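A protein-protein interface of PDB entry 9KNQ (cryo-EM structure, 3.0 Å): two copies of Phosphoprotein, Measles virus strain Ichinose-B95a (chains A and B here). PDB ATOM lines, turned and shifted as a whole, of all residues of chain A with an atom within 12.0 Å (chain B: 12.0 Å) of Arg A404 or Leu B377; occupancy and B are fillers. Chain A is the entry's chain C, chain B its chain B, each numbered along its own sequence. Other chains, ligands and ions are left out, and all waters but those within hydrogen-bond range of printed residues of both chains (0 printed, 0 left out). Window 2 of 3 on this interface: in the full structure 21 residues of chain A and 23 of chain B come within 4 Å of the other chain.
O of Met B371 sits at hydrogen-bond distance from N of Ile A398, 3.0 Å away.
The backbone NH (N) of Ala B373 lies within hydrogen-bond range of the backbone carbonyl oxygen (O) of Ile A398 (2.9 Å).
The guanidinium group (NH2) of Arg A404 lies within hydrogen-bond range of the backbone carbonyl oxygen (O) of Leu B377, at 2.7 Å.
Of the 10 printed residues of chain B, 5 touch a printed residue of chain A.
Hydrophobic or aromatic side chains of chain B within 4 Å of the printed part of chain A: Met B371, Ala B373 and Pro B375.
Hydrophobic or aromatic side chains of chain A that line the printed part of chain B: Ile A397 and Ile A398.
Among the printed residues, 8 pairs touch across the chains.
The side-chain carboxylate of Asp A401 is in salt-bridge range of the guanidinium group of Arg A404, 3.8 Å away.
No position is printed for both chains.
Printed residues of chain B within 4 Å of Ile A397: Met B371.
No residue of chain B comes within 4 Å of Asp A401.
No residue of chain B comes within 4 Å of Gly A403.
No residue of chain B comes within 4 Å of Ala A405.
No residue of chain B comes within 4 Å of Leu A406.
Ala A407 touches none of the printed residues of chain B.
Glu A408 touches none of the printed residues of chain B.
Leu A410 touches none of the printed residues of chain B.
Of the printed residues of chain A, Ile B372 touches Ile A398.
Ala B373 touches just these residues of chain A: Ile A398 (2.9 Å), Gly A399 (3.6 Å) and Arg A400 (3.7 Å).
Pro B375 touches just one residue of chain A: Arg A404 (3.5 Å).
Gly B376 touches none of the printed residues of chain A.
Leu B377 touches just one residue of chain A: Arg A404.
Gly B378 touches none of the printed residues of chain A.
No residue of chain A comes within 4 Å of Asp B380.
The nearest residue of chain B that does not touch Arg A404 is Asp B380 (4.2 Å).
The nearest residue of chain A that does not touch Leu B377 is Arg A400 (6.2 Å).
O of Met B371 touches CA of Ile A397, 3.3 Å away.
Ile A398 touches Ile B372.
CA of Gly A399 touches O of Ala B373, at 3.6 Å.
N of Arg A400 touches O of Ala B373, at 3.7 Å.
Arg A404 touches Pro B375 (NH2 to CB, 3.5 Å).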
ATOM      1  N   ILE A 370     -33.688 -38.491  31.876  1.00  0.00           N
ATOM      2  CA  ILE A 370     -32.579 -37.766  31.267  1.00  0.00           C
ATOM      3  C   ILE A 370     -32.980 -37.058  29.978  1.00  0.00           C
ATOM      4  O   ILE A 370     -32.353 -36.057  29.615  1.00  0.00           O
ATOM      5  CB  ILE A 370     -31.380 -38.700  31.010  1.00  0.00           C
ATOM      6  CG1 ILE A 370     -30.110 -37.879  30.786  1.00  0.00           C
ATOM      7  CG2 ILE A 370     -31.625 -39.559  29.797  1.00  0.00           C
ATOM      8  CD1 ILE A 370     -29.937 -36.729  31.757  1.00  0.00           C
ATOM      9  N   ILE A 397     -28.955 -37.515  26.629  1.00  0.00           N
ATOM     10  CA  ILE A 397     -27.836 -36.590  26.504  1.00  0.00           C
ATOM     11  C   ILE A 397     -27.203 -36.382  27.873  1.00  0.00           C
ATOM     12  O   ILE A 397     -27.877 -36.434  28.906  1.00  0.00           O
ATOM     13  CB  ILE A 397     -28.283 -35.252  25.870  1.00  0.00           C
ATOM     14  CG1 ILE A 397     -27.230 -34.753  24.883  1.00  0.00           C
ATOM     15  CG2 ILE A 397     -28.558 -34.202  26.932  1.00  0.00           C
ATOM     16  CD1 ILE A 397     -27.749 -33.713  23.924  1.00  0.00           C
ATOM     17  N   ILE A 398     -25.885 -36.168  27.872  1.00  0.00           N
ATOM     18  CA  ILE A 398     -25.118 -35.904  29.083  1.00  0.00           C
ATOM     19  C   ILE A 398     -23.991 -34.947  28.726  1.00  0.00           C
ATOM     20  O   ILE A 398     -23.645 -34.771  27.556  1.00  0.00           O
ATOM     21  CB  ILE A 398     -24.542 -37.191  29.717  1.00  0.00           C
ATOM     22  CG1 ILE A 398     -23.987 -38.114  28.634  1.00  0.00           C
ATOM     23  CG2 ILE A 398     -25.596 -37.901  30.545  1.00  0.00           C
ATOM     24  CD1 ILE A 398     -23.478 -39.431  29.164  1.00  0.00           C
ATOM     25  N   GLY A 399     -23.406 -34.325  29.753  1.00  0.00           N
ATOM     26  CA  GLY A 399     -22.390 -33.319  29.551  1.00  0.00           C
ATOM     27  C   GLY A 399     -21.175 -33.565  30.428  1.00  0.00           C
ATOM     28  O   GLY A 399     -21.169 -34.447  31.288  1.00  0.00           O
ATOM     29  N   ARG A 400     -20.135 -32.763  30.177  1.00  0.00           N
ATOM     30  CA  ARG A 400     -18.898 -32.867  30.943  1.00  0.00           C
ATOM     31  C   ARG A 400     -19.175 -32.781  32.436  1.00  0.00           C
ATOM     32  O   ARG A 400     -18.793 -33.667  33.208  1.00  0.00           O
ATOM     33  CB  ARG A 400     -17.929 -31.768  30.515  1.00  0.00           C
ATOM     34  CG  ARG A 400     -16.782 -31.555  31.475  1.00  0.00           C
ATOM     35  CD  ARG A 400     -15.750 -30.620  30.884  1.00  0.00           C
ATOM     36  NE  ARG A 400     -15.274 -31.091  29.590  1.00  0.00           N
ATOM     37  CZ  ARG A 400     -14.091 -30.782  29.076  1.00  0.00           C
ATOM     38  NH1 ARG A 400     -13.260 -30.004  29.752  1.00  0.00           N
ATOM     39  NH2 ARG A 400     -13.737 -31.252  27.891  1.00  0.00           N
ATOM     40  N   ASP A 401     -19.835 -31.715  32.860  1.00  0.00           N
ATOM     41  CA  ASP A 401     -20.393 -31.611  34.197  1.00  0.00           C
ATOM     42  C   ASP A 401     -21.913 -31.647  34.080  1.00  0.00           C
ATOM     43  O   ASP A 401     -22.468 -31.811  32.991  1.00  0.00           O
ATOM     44  CB  ASP A 401     -19.892 -30.347  34.898  1.00  0.00           C
ATOM     45  CG  ASP A 401     -18.391 -30.335  35.063  1.00  0.00           C
ATOM     46  OD1 ASP A 401     -17.735 -31.285  34.589  1.00  0.00           O
ATOM     47  OD2 ASP A 401     -17.863 -29.379  35.668  1.00  0.00           O
ATOM     48  N   SER A 402     -22.589 -31.502  35.216  1.00  0.00           N
ATOM     49  CA  SER A 402     -24.044 -31.532  35.217  1.00  0.00           C
ATOM     50  C   SER A 402     -24.614 -30.373  34.407  1.00  0.00           C
ATOM     51  O   SER A 402     -25.230 -30.583  33.357  1.00  0.00           O
ATOM     52  CB  SER A 402     -24.571 -31.492  36.651  1.00  0.00           C
ATOM     53  OG  SER A 402     -23.712 -32.202  37.525  1.00  0.00           O
ATOM     54  N   GLY A 403     -24.394 -29.150  34.880  1.00  0.00           N
ATOM     55  CA  GLY A 403     -24.968 -27.972  34.262  1.00  0.00           C
ATOM     56  C   GLY A 403     -24.095 -27.275  33.238  1.00  0.00           C
ATOM     57  O   GLY A 403     -23.694 -26.127  33.448  1.00  0.00           O
ATOM     58  N   ARG A 404     -23.782 -27.947  32.131  1.00  0.00           N
ATOM     59  CA  ARG A 404     -23.041 -27.319  31.044  1.00  0.00           C
ATOM     60  C   ARG A 404     -23.663 -27.649  29.692  1.00  0.00           C
ATOM     61  O   ARG A 404     -22.965 -27.719  28.678  1.00  0.00           O
ATOM     62  CB  ARG A 404     -21.568 -27.727  31.075  1.00  0.00           C
ATOM     63  CG  ARG A 404     -20.894 -27.530  32.426  1.00  0.00           C
ATOM     64  CD  ARG A 404     -20.518 -26.075  32.658  1.00  0.00           C
ATOM     65  NE  ARG A 404     -19.421 -25.642  31.797  1.00  0.00           N
ATOM     66  CZ  ARG A 404     -18.134 -25.827  32.074  1.00  0.00           C
ATOM     67  NH1 ARG A 404     -17.776 -26.439  33.193  1.00  0.00           N
ATOM     68  NH2 ARG A 404     -17.206 -25.401  31.231  1.00  0.00           N
ATOM     69  N   ALA A 405     -24.981 -27.850  29.665  1.00  0.00           N
ATOM     70  CA  ALA A 405     -25.703 -28.158  28.440  1.00  0.00           C
ATOM     71  C   ALA A 405     -26.688 -27.076  28.030  1.00  0.00           C
ATOM     72  O   ALA A 405     -27.296 -27.191  26.961  1.00  0.00           O
ATOM     73  CB  ALA A 405     -26.454 -29.490  28.584  1.00  0.00           C
ATOM     74  N   LEU A 406     -26.865 -26.034  28.840  1.00  0.00           N
ATOM     75  CA  LEU A 406     -27.847 -24.996  28.554  1.00  0.00           C
ATOM     76  C   LEU A 406     -27.441 -24.079  27.407  1.00  0.00           C
ATOM     77  O   LEU A 406     -28.150 -23.102  27.147  1.00  0.00           O
ATOM     78  CB  LEU A 406     -28.102 -24.163  29.811  1.00  0.00           C
ATOM     79  CG  LEU A 406     -26.861 -23.738  30.595  1.00  0.00           C
ATOM     80  CD1 LEU A 406     -26.361 -22.375  30.137  1.00  0.00           C
ATOM     81  CD2 LEU A 406     -27.148 -23.734  32.088  1.00  0.00           C
ATOM     82  N   ALA A 407     -26.331 -24.355  26.726  1.00  0.00           N
ATOM     83  CA  ALA A 407     -25.905 -23.544  25.597  1.00  0.00           C
ATOM     84  C   ALA A 407     -26.204 -24.191  24.253  1.00  0.00           C
ATOM     85  O   ALA A 407     -25.975 -23.560  23.216  1.00  0.00           O
ATOM     86  CB  ALA A 407     -24.404 -23.248  25.694  1.00  0.00           C
ATOM     87  N   GLU A 408     -26.704 -25.428  24.244  1.00  0.00           N
ATOM     88  CA  GLU A 408     -26.972 -26.120  22.992  1.00  0.00           C
ATOM     89  C   GLU A 408     -28.277 -26.907  23.013  1.00  0.00           C
ATOM     90  O   GLU A 408     -28.504 -27.718  22.107  1.00  0.00           O
ATOM     91  CB  GLU A 408     -25.813 -27.062  22.647  1.00  0.00           C
ATOM     92  CG  GLU A 408     -24.745 -26.431  21.770  1.00  0.00           C
ATOM     93  CD  GLU A 408     -25.138 -26.408  20.309  1.00  0.00           C
ATOM     94  OE1 GLU A 408     -26.168 -27.017  19.973  1.00  0.00           O
ATOM     95  OE2 GLU A 408     -24.418 -25.784  19.501  1.00  0.00           O
ATOM     96  N   VAL A 409     -29.139 -26.703  24.008  1.00  0.00           N
ATOM     97  CA  VAL A 409     -30.318 -27.544  24.170  1.00  0.00           C
ATOM     98  C   VAL A 409     -31.609 -26.882  23.695  1.00  0.00           C
ATOM     99  O   VAL A 409     -32.595 -27.593  23.446  1.00  0.00           O
ATOM    100  CB  VAL A 409     -30.465 -27.994  25.641  1.00  0.00           C
ATOM    101  CG1 VAL A 409     -31.169 -26.925  26.463  1.00  0.00           C
ATOM    102  CG2 VAL A 409     -31.202 -29.320  25.725  1.00  0.00           C
ATOM    103  N   LEU A 410     -31.639 -25.560  23.557  1.00  0.00           N
ATOM    104  CA  LEU A 410     -32.859 -24.869  23.163  1.00  0.00           C
ATOM    105  C   LEU A 410     -32.697 -23.963  21.953  1.00  0.00           C
ATOM    106  O   LEU A 410     -33.647 -23.829  21.178  1.00  0.00           O
ATOM    107  CB  LEU A 410     -33.403 -24.036  24.334  1.00  0.00           C
ATOM    108  CG  LEU A 410     -34.708 -23.275  24.090  1.00  0.00           C
ATOM    109  CD1 LEU A 410     -35.816 -24.233  23.690  1.00  0.00           C
ATOM    110  CD2 LEU A 410     -35.104 -22.468  25.318  1.00  0.00           C
ATOM    111  N   LYS A 411     -31.529 -23.352  21.768  1.00  0.00           N
ATOM    112  CA  LYS A 411     -31.308 -22.365  20.710  1.00  0.00           C
ATOM    113  C   LYS A 411     -32.315 -21.221  20.801  1.00  0.00           C
ATOM    114  O   LYS A 411     -32.683 -20.622  19.791  1.00  0.00           O
ATOM    115  CB  LYS A 411     -31.376 -23.017  19.328  1.00  0.00           C
ATOM    116  CG  LYS A 411     -30.033 -23.451  18.775  1.00  0.00           C
ATOM    117  CD  LYS A 411     -29.940 -23.182  17.278  1.00  0.00           C
ATOM    118  CE  LYS A 411     -31.211 -23.600  16.550  1.00  0.00           C
ATOM    119  NZ  LYS A 411     -31.029 -23.640  15.075  1.00  0.00           N
ATOM    120  N   LYS A 435     -33.012 -29.008  20.141  1.00  0.00           N
ATOM    121  CA  LYS A 435     -31.652 -28.642  20.518  1.00  0.00           C
ATOM    122  C   LYS A 435     -31.060 -27.515  19.676  1.00  0.00           C
ATOM    123  O   LYS A 435     -30.828 -26.417  20.190  1.00  0.00           O
ATOM    124  CB  LYS A 435     -30.744 -29.868  20.429  1.00  0.00           C
ATOM    125  CG  LYS A 435     -31.142 -30.848  19.348  1.00  0.00           C
ATOM    126  CD  LYS A 435     -30.109 -31.946  19.222  1.00  0.00           C
ATOM    127  CE  LYS A 435     -28.814 -31.412  18.648  1.00  0.00           C
ATOM    128  NZ  LYS A 435     -28.975 -31.003  17.230  1.00  0.00           N
ATOM    129  N   GLU A 436     -30.819 -27.762  18.392  1.00  0.00           N
ATOM    130  CA  GLU A 436     -30.103 -26.798  17.564  1.00  0.00           C
ATOM    131  C   GLU A 436     -30.287 -27.163  16.095  1.00  0.00           C
ATOM    132  O   GLU A 436     -31.115 -28.007  15.741  1.00  0.00           O
ATOM    133  CB  GLU A 436     -28.617 -26.746  17.940  1.00  0.00           C
ATOM    134  CG  GLU A 436     -27.798 -27.940  17.448  1.00  0.00           C
ATOM    135  CD  GLU A 436     -26.388 -27.556  17.032  1.00  0.00           C
ATOM    136  OE1 GLU A 436     -25.993 -26.394  17.254  1.00  0.00           O
ATOM    137  OE2 GLU A 436     -25.675 -28.418  16.477  1.00  0.00           O
ATOM    138  N   MET B 371     -25.819 -39.157  23.481  1.00  0.00           N
ATOM    139  CA  MET B 371     -25.166 -37.982  22.924  1.00  0.00           C
ATOM    140  C   MET B 371     -24.430 -37.226  24.019  1.00  0.00           C
ATOM    141  O   MET B 371     -24.914 -37.122  25.148  1.00  0.00           O
ATOM    142  CB  MET B 371     -26.178 -37.061  22.243  1.00  0.00           C
ATOM    143  CG  MET B 371     -26.665 -37.578  20.904  1.00  0.00           C
ATOM    144  SD  MET B 371     -27.636 -36.363  20.000  1.00  0.00           S
ATOM    145  CE  MET B 371     -27.659 -37.107  18.373  1.00  0.00           C
ATOM    146  N   ILE B 372     -23.259 -36.697  23.675  1.00  0.00           N
ATOM    147  CA  ILE B 372     -22.397 -35.984  24.609  1.00  0.00           C
ATOM    148  C   ILE B 372     -22.341 -34.521  24.195  1.00  0.00           C
ATOM    149  O   ILE B 372     -22.181 -34.212  23.009  1.00  0.00           O
ATOM    150  CB  ILE B 372     -20.988 -36.595  24.647  1.00  0.00           C
ATOM    151  CG1 ILE B 372     -21.069 -38.108  24.838  1.00  0.00           C
ATOM    152  CG2 ILE B 372     -20.171 -35.971  25.754  1.00  0.00           C
ATOM    153  CD1 ILE B 372     -19.730 -38.797  24.775  1.00  0.00           C
ATOM    154  N   ALA B 373     -22.465 -33.625  25.169  1.00  0.00           N
ATOM    155  CA  ALA B 373     -22.411 -32.189  24.937  1.00  0.00           C
ATOM    156  C   ALA B 373     -21.123 -31.631  25.520  1.00  0.00           C
ATOM    157  O   ALA B 373     -20.742 -31.981  26.641  1.00  0.00           O
ATOM    158  CB  ALA B 373     -23.621 -31.488  25.558  1.00  0.00           C
ATOM    159  N   ILE B 374     -20.461 -30.767  24.765  1.00  0.00           N
ATOM    160  CA  ILE B 374     -19.166 -30.203  25.137  1.00  0.00           C
ATOM    161  C   ILE B 374     -19.348 -28.710  25.379  1.00  0.00           C
ATOM    162  O   ILE B 374     -19.935 -28.027  24.535  1.00  0.00           O
ATOM    163  CB  ILE B 374     -18.107 -30.448  24.049  1.00  0.00           C
ATOM    164  CG1 ILE B 374     -17.867 -31.947  23.878  1.00  0.00           C
ATOM    165  CG2 ILE B 374     -16.816 -29.735  24.388  1.00  0.00           C
ATOM    166  CD1 ILE B 374     -16.744 -32.274  22.934  1.00  0.00           C
ATOM    167  N   PRO B 375     -18.866 -28.170  26.490  1.00  0.00           N
ATOM    168  CA  PRO B 375     -19.044 -26.745  26.778  1.00  0.00           C
ATOM    169  C   PRO B 375     -18.124 -25.891  25.912  1.00  0.00           C
ATOM    170  O   PRO B 375     -17.383 -26.387  25.067  1.00  0.00           O
ATOM    171  CB  PRO B 375     -18.675 -26.644  28.256  1.00  0.00           C
ATOM    172  CG  PRO B 375     -17.698 -27.733  28.455  1.00  0.00           C
ATOM    173  CD  PRO B 375     -18.165 -28.863  27.583  1.00  0.00           C
ATOM    174  N   GLY B 376     -18.182 -24.582  26.144  1.00  0.00           N
ATOM    175  CA  GLY B 376     -17.393 -23.642  25.376  1.00  0.00           C
ATOM    176  C   GLY B 376     -16.117 -23.201  26.060  1.00  0.00           C
ATOM    177  O   GLY B 376     -15.052 -23.175  25.436  1.00  0.00           O
ATOM    178  N   LEU B 377     -16.203 -22.849  27.339  1.00  0.00           N
ATOM    179  CA  LEU B 377     -15.053 -22.389  28.105  1.00  0.00           C
ATOM    180  C   LEU B 377     -14.551 -23.513  29.000  1.00  0.00           C
ATOM    181  O   LEU B 377     -15.336 -24.141  29.718  1.00  0.00           O
ATOM    182  CB  LEU B 377     -15.411 -21.165  28.946  1.00  0.00           C
ATOM    183  CG  LEU B 377     -15.651 -19.883  28.155  1.00  0.00           C
ATOM    184  CD1 LEU B 377     -15.637 -18.681  29.081  1.00  0.00           C
ATOM    185  CD2 LEU B 377     -14.612 -19.733  27.060  1.00  0.00           C
ATOM    186  N   GLY B 378     -13.241 -23.755  28.961  1.00  0.00           N
ATOM    187  CA  GLY B 378     -12.675 -24.890  29.662  1.00  0.00           C
ATOM    188  C   GLY B 378     -12.695 -24.780  31.171  1.00  0.00           C
ATOM    189  O   GLY B 378     -12.535 -25.797  31.853  1.00  0.00           O
ATOM    190  N   LYS B 379     -12.882 -23.584  31.712  1.00  0.00           N
ATOM    191  CA  LYS B 379     -12.834 -23.417  33.159  1.00  0.00           C
ATOM    192  C   LYS B 379     -14.100 -22.828  33.754  1.00  0.00           C
ATOM    193  O   LYS B 379     -14.536 -23.281  34.815  1.00  0.00           O
ATOM    194  CB  LYS B 379     -11.641 -22.535  33.546  1.00  0.00           C
ATOM    195  CG  LYS B 379     -11.330 -22.545  35.030  1.00  0.00           C
ATOM    196  CD  LYS B 379     -11.441 -21.153  35.619  1.00  0.00           C
ATOM    197  CE  LYS B 379     -11.125 -21.157  37.103  1.00  0.00           C
ATOM    198  NZ  LYS B 379     -11.374 -19.826  37.719  1.00  0.00           N
ATOM    199  N   ASP B 380     -14.705 -21.842  33.096  1.00  0.00           N
ATOM    200  CA  ASP B 380     -15.855 -21.114  33.633  1.00  0.00           C
ATOM    201  C   ASP B 380     -15.558 -20.532  35.014  1.00  0.00           C
ATOM    202  O   ASP B 380     -15.841 -21.153  36.039  1.00  0.00           O
ATOM    203  CB  ASP B 380     -17.090 -22.015  33.702  1.00  0.00           C
ATOM    204  CG  ASP B 380     -18.275 -21.331  34.357  1.00  0.00           C
ATOM    205  OD1 ASP B 380     -18.862 -20.424  33.731  1.00  0.00           O
ATOM    206  OD2 ASP B 380     -18.614 -21.697  35.501  1.00  0.00           O
